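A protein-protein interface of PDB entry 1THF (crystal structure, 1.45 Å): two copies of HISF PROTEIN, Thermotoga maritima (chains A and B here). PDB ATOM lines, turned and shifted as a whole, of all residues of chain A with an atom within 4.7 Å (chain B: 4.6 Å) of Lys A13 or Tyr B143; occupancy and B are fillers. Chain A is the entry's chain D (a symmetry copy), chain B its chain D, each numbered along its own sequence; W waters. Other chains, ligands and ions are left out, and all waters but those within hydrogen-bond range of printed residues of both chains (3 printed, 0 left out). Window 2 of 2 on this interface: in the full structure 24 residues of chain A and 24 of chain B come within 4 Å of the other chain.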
ATOM      1  N   ASP A  11     -13.436  14.451  29.920  1.00  0.00           N
ATOM      2  CA  ASP A  11     -12.256  15.140  29.394  1.00  0.00           C
ATOM      3  C   ASP A  11     -11.355  14.121  28.712  1.00  0.00           C
ATOM      4  O   ASP A  11     -11.043  13.084  29.296  1.00  0.00           O
ATOM      5  CB  ASP A  11     -11.566  15.878  30.538  1.00  0.00           C
ATOM      6  CG  ASP A  11     -12.390  17.059  31.014  1.00  0.00           C
ATOM      7  OD1 ASP A  11     -13.471  17.368  30.486  1.00  0.00           O
ATOM      8  OD2 ASP A  11     -11.928  17.712  31.979  1.00  0.00           O
ATOM      9  N   VAL A  12     -10.958  14.416  27.487  1.00  0.00           N
ATOM     10  CA  VAL A  12     -10.153  13.546  26.652  1.00  0.00           C
ATOM     11  C   VAL A  12      -8.759  14.085  26.366  1.00  0.00           C
ATOM     12  O   VAL A  12      -8.555  15.271  26.149  1.00  0.00           O
ATOM     13  CB  VAL A  12     -10.893  13.325  25.304  1.00  0.00           C
ATOM     14  CG1 VAL A  12     -10.049  12.600  24.268  1.00  0.00           C
ATOM     15  CG2 VAL A  12     -12.192  12.556  25.517  1.00  0.00           C
ATOM     16  N   LYS A  13      -7.793  13.184  26.372  1.00  0.00           N
ATOM     17  CA  LYS A  13      -6.405  13.448  26.029  1.00  0.00           C
ATOM     18  C   LYS A  13      -5.929  12.255  25.189  1.00  0.00           C
ATOM     19  O   LYS A  13      -6.030  11.104  25.606  1.00  0.00           O
ATOM     20  CB  LYS A  13      -5.475  13.605  27.228  1.00  0.00           C
ATOM     21  CG  LYS A  13      -3.991  13.604  26.843  1.00  0.00           C
ATOM     22  CD  LYS A  13      -3.100  13.811  28.059  1.00  0.00           C
ATOM     23  CE  LYS A  13      -1.625  13.678  27.710  1.00  0.00           C
ATOM     24  NZ  LYS A  13      -1.236  12.263  27.449  1.00  0.00           N
ATOM     25  N   ASP A  14      -5.444  12.532  23.984  1.00  0.00           N
ATOM     26  CA  ASP A  14      -4.953  11.508  23.070  1.00  0.00           C
ATOM     27  C   ASP A  14      -5.976  10.411  22.791  1.00  0.00           C
ATOM     28  O   ASP A  14      -5.665   9.215  22.723  1.00  0.00           O
ATOM     29  CB  ASP A  14      -3.647  10.895  23.591  1.00  0.00           C
ATOM     30  CG  ASP A  14      -2.537  11.889  23.843  1.00  0.00           C
ATOM     31  OD1 ASP A  14      -2.449  12.900  23.118  1.00  0.00           O
ATOM     32  OD2 ASP A  14      -1.731  11.683  24.783  1.00  0.00           O
ATOM     33  N   GLY A  15      -7.243  10.779  22.650  1.00  0.00           N
ATOM     34  CA  GLY A  15      -8.330   9.874  22.339  1.00  0.00           C
ATOM     35  C   GLY A  15      -8.821   9.002  23.471  1.00  0.00           C
ATOM     36  O   GLY A  15      -9.595   8.063  23.238  1.00  0.00           O
ATOM     37  N   ARG A  16      -8.365   9.235  24.693  1.00  0.00           N
ATOM     38  CA  ARG A  16      -8.778   8.466  25.857  1.00  0.00           C
ATOM     39  C   ARG A  16      -9.266   9.411  26.956  1.00  0.00           C
ATOM     40  O   ARG A  16      -8.821  10.557  27.040  1.00  0.00           O
ATOM     41  CB  ARG A  16      -7.641   7.602  26.394  1.00  0.00           C
ATOM     42  CG  ARG A  16      -7.091   6.594  25.394  1.00  0.00           C
ATOM     43  CD  ARG A  16      -6.057   5.691  26.038  1.00  0.00           C
ATOM     44  NE  ARG A  16      -6.602   4.916  27.133  1.00  0.00           N
ATOM     45  CZ  ARG A  16      -7.547   3.989  27.060  1.00  0.00           C
ATOM     46  NH1 ARG A  16      -8.147   3.649  25.930  1.00  0.00           N
ATOM     47  NH2 ARG A  16      -7.890   3.390  28.189  1.00  0.00           N
ATOM     48  N   VAL A  18      -9.445  11.060  30.467  1.00  0.00           N
ATOM     49  CA  VAL A  18      -8.517  11.268  31.581  1.00  0.00           C
ATOM     50  C   VAL A  18      -8.926  10.341  32.716  1.00  0.00           C
ATOM     51  O   VAL A  18     -10.109  10.277  33.074  1.00  0.00           O
ATOM     52  CB  VAL A  18      -8.523  12.745  32.005  1.00  0.00           C
ATOM     53  CG1 VAL A  18      -7.750  12.966  33.293  1.00  0.00           C
ATOM     54  CG2 VAL A  18      -7.942  13.580  30.869  1.00  0.00           C
ATOM     55  N   ILE A  52      -9.096  18.289  26.016  1.00  0.00           N
ATOM     56  CA  ILE A  52      -8.531  19.345  26.854  1.00  0.00           C
ATOM     57  C   ILE A  52      -7.123  19.783  26.496  1.00  0.00           C
ATOM     58  O   ILE A  52      -6.543  20.647  27.151  1.00  0.00           O
ATOM     59  CB  ILE A  52      -8.586  19.018  28.361  1.00  0.00           C
ATOM     60  CG1 ILE A  52      -7.748  17.784  28.680  1.00  0.00           C
ATOM     61  CG2 ILE A  52     -10.046  18.870  28.758  1.00  0.00           C
ATOM     62  CD1 ILE A  52      -7.569  17.484  30.153  1.00  0.00           C
ATOM     63  N   THR A  53      -6.557  19.101  25.526  1.00  0.00           N
ATOM     64  CA  THR A  53      -5.297  19.514  24.915  1.00  0.00           C
ATOM     65  C   THR A  53      -5.771  20.321  23.704  1.00  0.00           C
ATOM     66  O   THR A  53      -5.440  21.463  23.455  1.00  0.00           O
ATOM     67  CB  THR A  53      -4.452  18.316  24.488  1.00  0.00           C
ATOM     68  OG1 THR A  53      -4.987  17.742  23.291  1.00  0.00           O
ATOM     69  CG2 THR A  53      -4.448  17.233  25.562  1.00  0.00           C
ATOM     70  N   THR B 104       1.849  22.338  32.967  1.00  0.00           N
ATOM     71  CA  THR B 104       1.407  20.943  32.849  1.00  0.00           C
ATOM     72  C   THR B 104       2.575  19.995  32.681  1.00  0.00           C
ATOM     73  O   THR B 104       2.598  18.925  33.288  1.00  0.00           O
ATOM     74  CB  THR B 104       0.486  20.802  31.626  1.00  0.00           C
ATOM     75  OG1 THR B 104      -0.644  21.659  31.836  1.00  0.00           O
ATOM     76  CG2 THR B 104       0.044  19.352  31.451  1.00  0.00           C
ATOM     77  N   GLU B 108       3.521  16.773  35.198  1.00  0.00           N
ATOM     78  CA  GLU B 108       3.630  15.417  34.649  1.00  0.00           C
ATOM     79  C   GLU B 108       5.013  14.828  34.678  1.00  0.00           C
ATOM     80  O   GLU B 108       5.198  13.610  34.527  1.00  0.00           O
ATOM     81  CB  GLU B 108       3.043  15.445  33.228  1.00  0.00           C
ATOM     82  CG  GLU B 108       1.534  15.658  33.360  1.00  0.00           C
ATOM     83  CD  GLU B 108       0.794  15.694  32.046  1.00  0.00           C
ATOM     84  OE1 GLU B 108       1.458  15.759  30.994  1.00  0.00           O
ATOM     85  OE2 GLU B 108      -0.462  15.716  32.119  1.00  0.00           O
ATOM     86  N   THR B 142      -4.237  21.623  35.770  1.00  0.00           N
ATOM     87  CA  THR B 142      -3.425  21.602  34.562  1.00  0.00           C
ATOM     88  C   THR B 142      -4.325  21.718  33.326  1.00  0.00           C
ATOM     89  O   THR B 142      -5.538  21.840  33.466  1.00  0.00           O
ATOM     90  CB  THR B 142      -2.532  20.353  34.469  1.00  0.00           C
ATOM     91  OG1 THR B 142      -3.325  19.188  34.705  1.00  0.00           O
ATOM     92  CG2 THR B 142      -1.425  20.447  35.525  1.00  0.00           C
ATOM     93  N   TYR B 143      -3.719  21.702  32.145  1.00  0.00           N
ATOM     94  CA  TYR B 143      -4.458  21.810  30.889  1.00  0.00           C
ATOM     95  C   TYR B 143      -5.339  23.046  30.835  1.00  0.00           C
ATOM     96  O   TYR B 143      -6.553  22.938  30.689  1.00  0.00           O
ATOM     97  CB  TYR B 143      -5.271  20.525  30.610  1.00  0.00           C
ATOM     98  CG  TYR B 143      -4.340  19.342  30.403  1.00  0.00           C
ATOM     99  CD1 TYR B 143      -3.764  19.093  29.165  1.00  0.00           C
ATOM    100  CD2 TYR B 143      -4.008  18.495  31.459  1.00  0.00           C
ATOM    101  CE1 TYR B 143      -2.891  18.041  28.970  1.00  0.00           C
ATOM    102  CE2 TYR B 143      -3.144  17.438  31.267  1.00  0.00           C
ATOM    103  CZ  TYR B 143      -2.591  17.220  30.029  1.00  0.00           C
ATOM    104  OH  TYR B 143      -1.716  16.159  29.882  1.00  0.00           O
ATOM    105  N   SER B 144      -4.742  24.220  31.006  1.00  0.00           N
ATOM    106  CA  SER B 144      -5.499  25.478  30.966  1.00  0.00           C
ATOM    107  C   SER B 144      -6.704  25.478  31.881  1.00  0.00           C
ATOM    108  O   SER B 144      -7.817  25.879  31.521  1.00  0.00           O
ATOM    109  CB  SER B 144      -5.937  25.769  29.514  1.00  0.00           C
ATOM    110  OG  SER B 144      -4.800  25.932  28.692  1.00  0.00           O
ATOM    111  N   GLY B 145      -6.529  25.062  33.139  1.00  0.00           N
ATOM    112  CA  GLY B 145      -7.577  25.003  34.128  1.00  0.00           C
ATOM    113  C   GLY B 145      -8.681  24.002  33.930  1.00  0.00           C
ATOM    114  O   GLY B 145      -9.708  24.039  34.622  1.00  0.00           O
ATOM    115  N   LYS B 146      -8.500  23.008  33.053  1.00  0.00           N
ATOM    116  CA  LYS B 146      -9.563  22.036  32.827  1.00  0.00           C
ATOM    117  C   LYS B 146      -9.349  20.715  33.539  1.00  0.00           C
ATOM    118  O   LYS B 146     -10.261  19.870  33.582  1.00  0.00           O
ATOM    119  CB  LYS B 146      -9.790  21.803  31.335  1.00  0.00           C
ATOM    120  CG  LYS B 146     -10.502  22.932  30.615  1.00  0.00           C
ATOM    121  CD  LYS B 146     -11.820  23.363  31.230  1.00  0.00           C
ATOM    122  CE  LYS B 146     -12.904  22.304  31.213  1.00  0.00           C
ATOM    123  NZ  LYS B 146     -14.265  22.866  31.493  1.00  0.00           N
ATOM    124  N   LYS B 147      -8.170  20.497  34.109  1.00  0.00           N
ATOM    125  CA  LYS B 147      -7.939  19.253  34.826  1.00  0.00           C
ATOM    126  C   LYS B 147      -7.571  19.502  36.291  1.00  0.00           C
ATOM    127  O   LYS B 147      -6.508  20.059  36.564  1.00  0.00           O
ATOM    128  CB  LYS B 147      -6.862  18.380  34.184  1.00  0.00           C
ATOM    129  CG  LYS B 147      -6.591  17.106  34.975  1.00  0.00           C
ATOM    130  CD  LYS B 147      -5.432  16.323  34.377  1.00  0.00           C
ATOM    131  CE  LYS B 147      -5.320  14.982  35.102  1.00  0.00           C
ATOM    132  NZ  LYS B 147      -4.133  14.229  34.583  1.00  0.00           N
HETATM  133  O   HOH W   1      -7.964  22.702  28.212  1.00  0.00           O
HETATM  134  O   HOH W   2     -10.209  16.671  33.765  1.00  0.00           O
HETATM  135  O   HOH W   3     -13.584  19.669  32.900  1.00  0.00           O
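The side-chain carboxylate (OD2) of Asp A11 sits close to the backbone carbonyl oxygen (O) of Lys B146, at 3.2 Å.
NZ of Lys A13 is in salt-bridge range of OD2 of Asp A14, 2.8 Å away. The side-chain carboxylate of Glu B108 is in hydrogen-bond range of the side-chain hydroxyl of Tyr B143. The backbone carbonyl oxygen of Lys B147 is in hydrogen-bond range of the backbone NH of Thr B142 (2.9 Å). N of Tyr B143 is in hydrogen-bond range of OG1 of Thr B104 (3.1 Å). The backbone carbonyl oxygen of Val A12 is in hydrogen-bond range of the backbone NH of Ile A52, 3.1 Å away. The backbone carbonyl oxygen (O) of Asp A11 is in hydrogen-bond range of the backbone NH (N) of Val A18, at 2.8 Å.
Among the printed residues, pairs that only touch across the chains: Lys A13 with Tyr B143, Val A18 with Lys B147, Ile A52 with Tyr B143, Thr A53 with Tyr B143 and Ile A52 with Lys B146.
Printed residues of chain B within 4 Å of Lys A13: Tyr B143 (3.3 Å). Tyr B143 touches just these residues of chain A: Lys A13, Ile A52 and Thr A53. Of the printed residues of chain B, Asp A11 touches Lys B146. Of the printed residues of chain B, Val A18 touches Lys B147. Printed residues of chain B within 4 Å of Thr A53: Tyr B143 (3.8 Å). Of the printed residues of chain A, Lys B147 touches Val A18 (3.6 Å). Printed residues of chain B within 4 Å of Ile A52: Tyr B143 and Lys B146. Thr B142 touches none of the printed residues of chain A. Glu B108 touches none of the printed residues of chain A. The nearest printed residue of chain A that does not touch Tyr B143 is Val A18 (6.2 Å). The nearest printed residue of chain B that does not touch Thr A53 is Ser B144 (6.9 Å).
Of the 9 printed residues of chain A, 5 touch a printed residue of chain B. Of the 8 printed residues of chain B, 3 touch a printed residue of chain A. Hydrophobic or aromatic side chains of chain B that line the printed part of chain A: Tyr B143. Among the printed residues, 6 pairs touch across the chains. Among the printed residues, no Asp or Glu carboxylate lies within 4 Å of a Lys or Arg side-chain nitrogen of the other chain.
No position is printed for both chains. Of the 6 pairs that touch across the chains among the printed residues, none has its exchanged pair printed and touching as well.
Water W2 lies within hydrogen-bond range of OD2 of Asp A11 (2.7 Å) and O of Lys B146 (3.2 Å). Water W1 lies within hydrogen-bond range of O of Ile A52 (2.7 Å) and O of Tyr B143 (2.9 Å). Water W3 bridges the side-chain carboxylate of Asp A11 and the backbone carbonyl oxygen of Lys B146.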
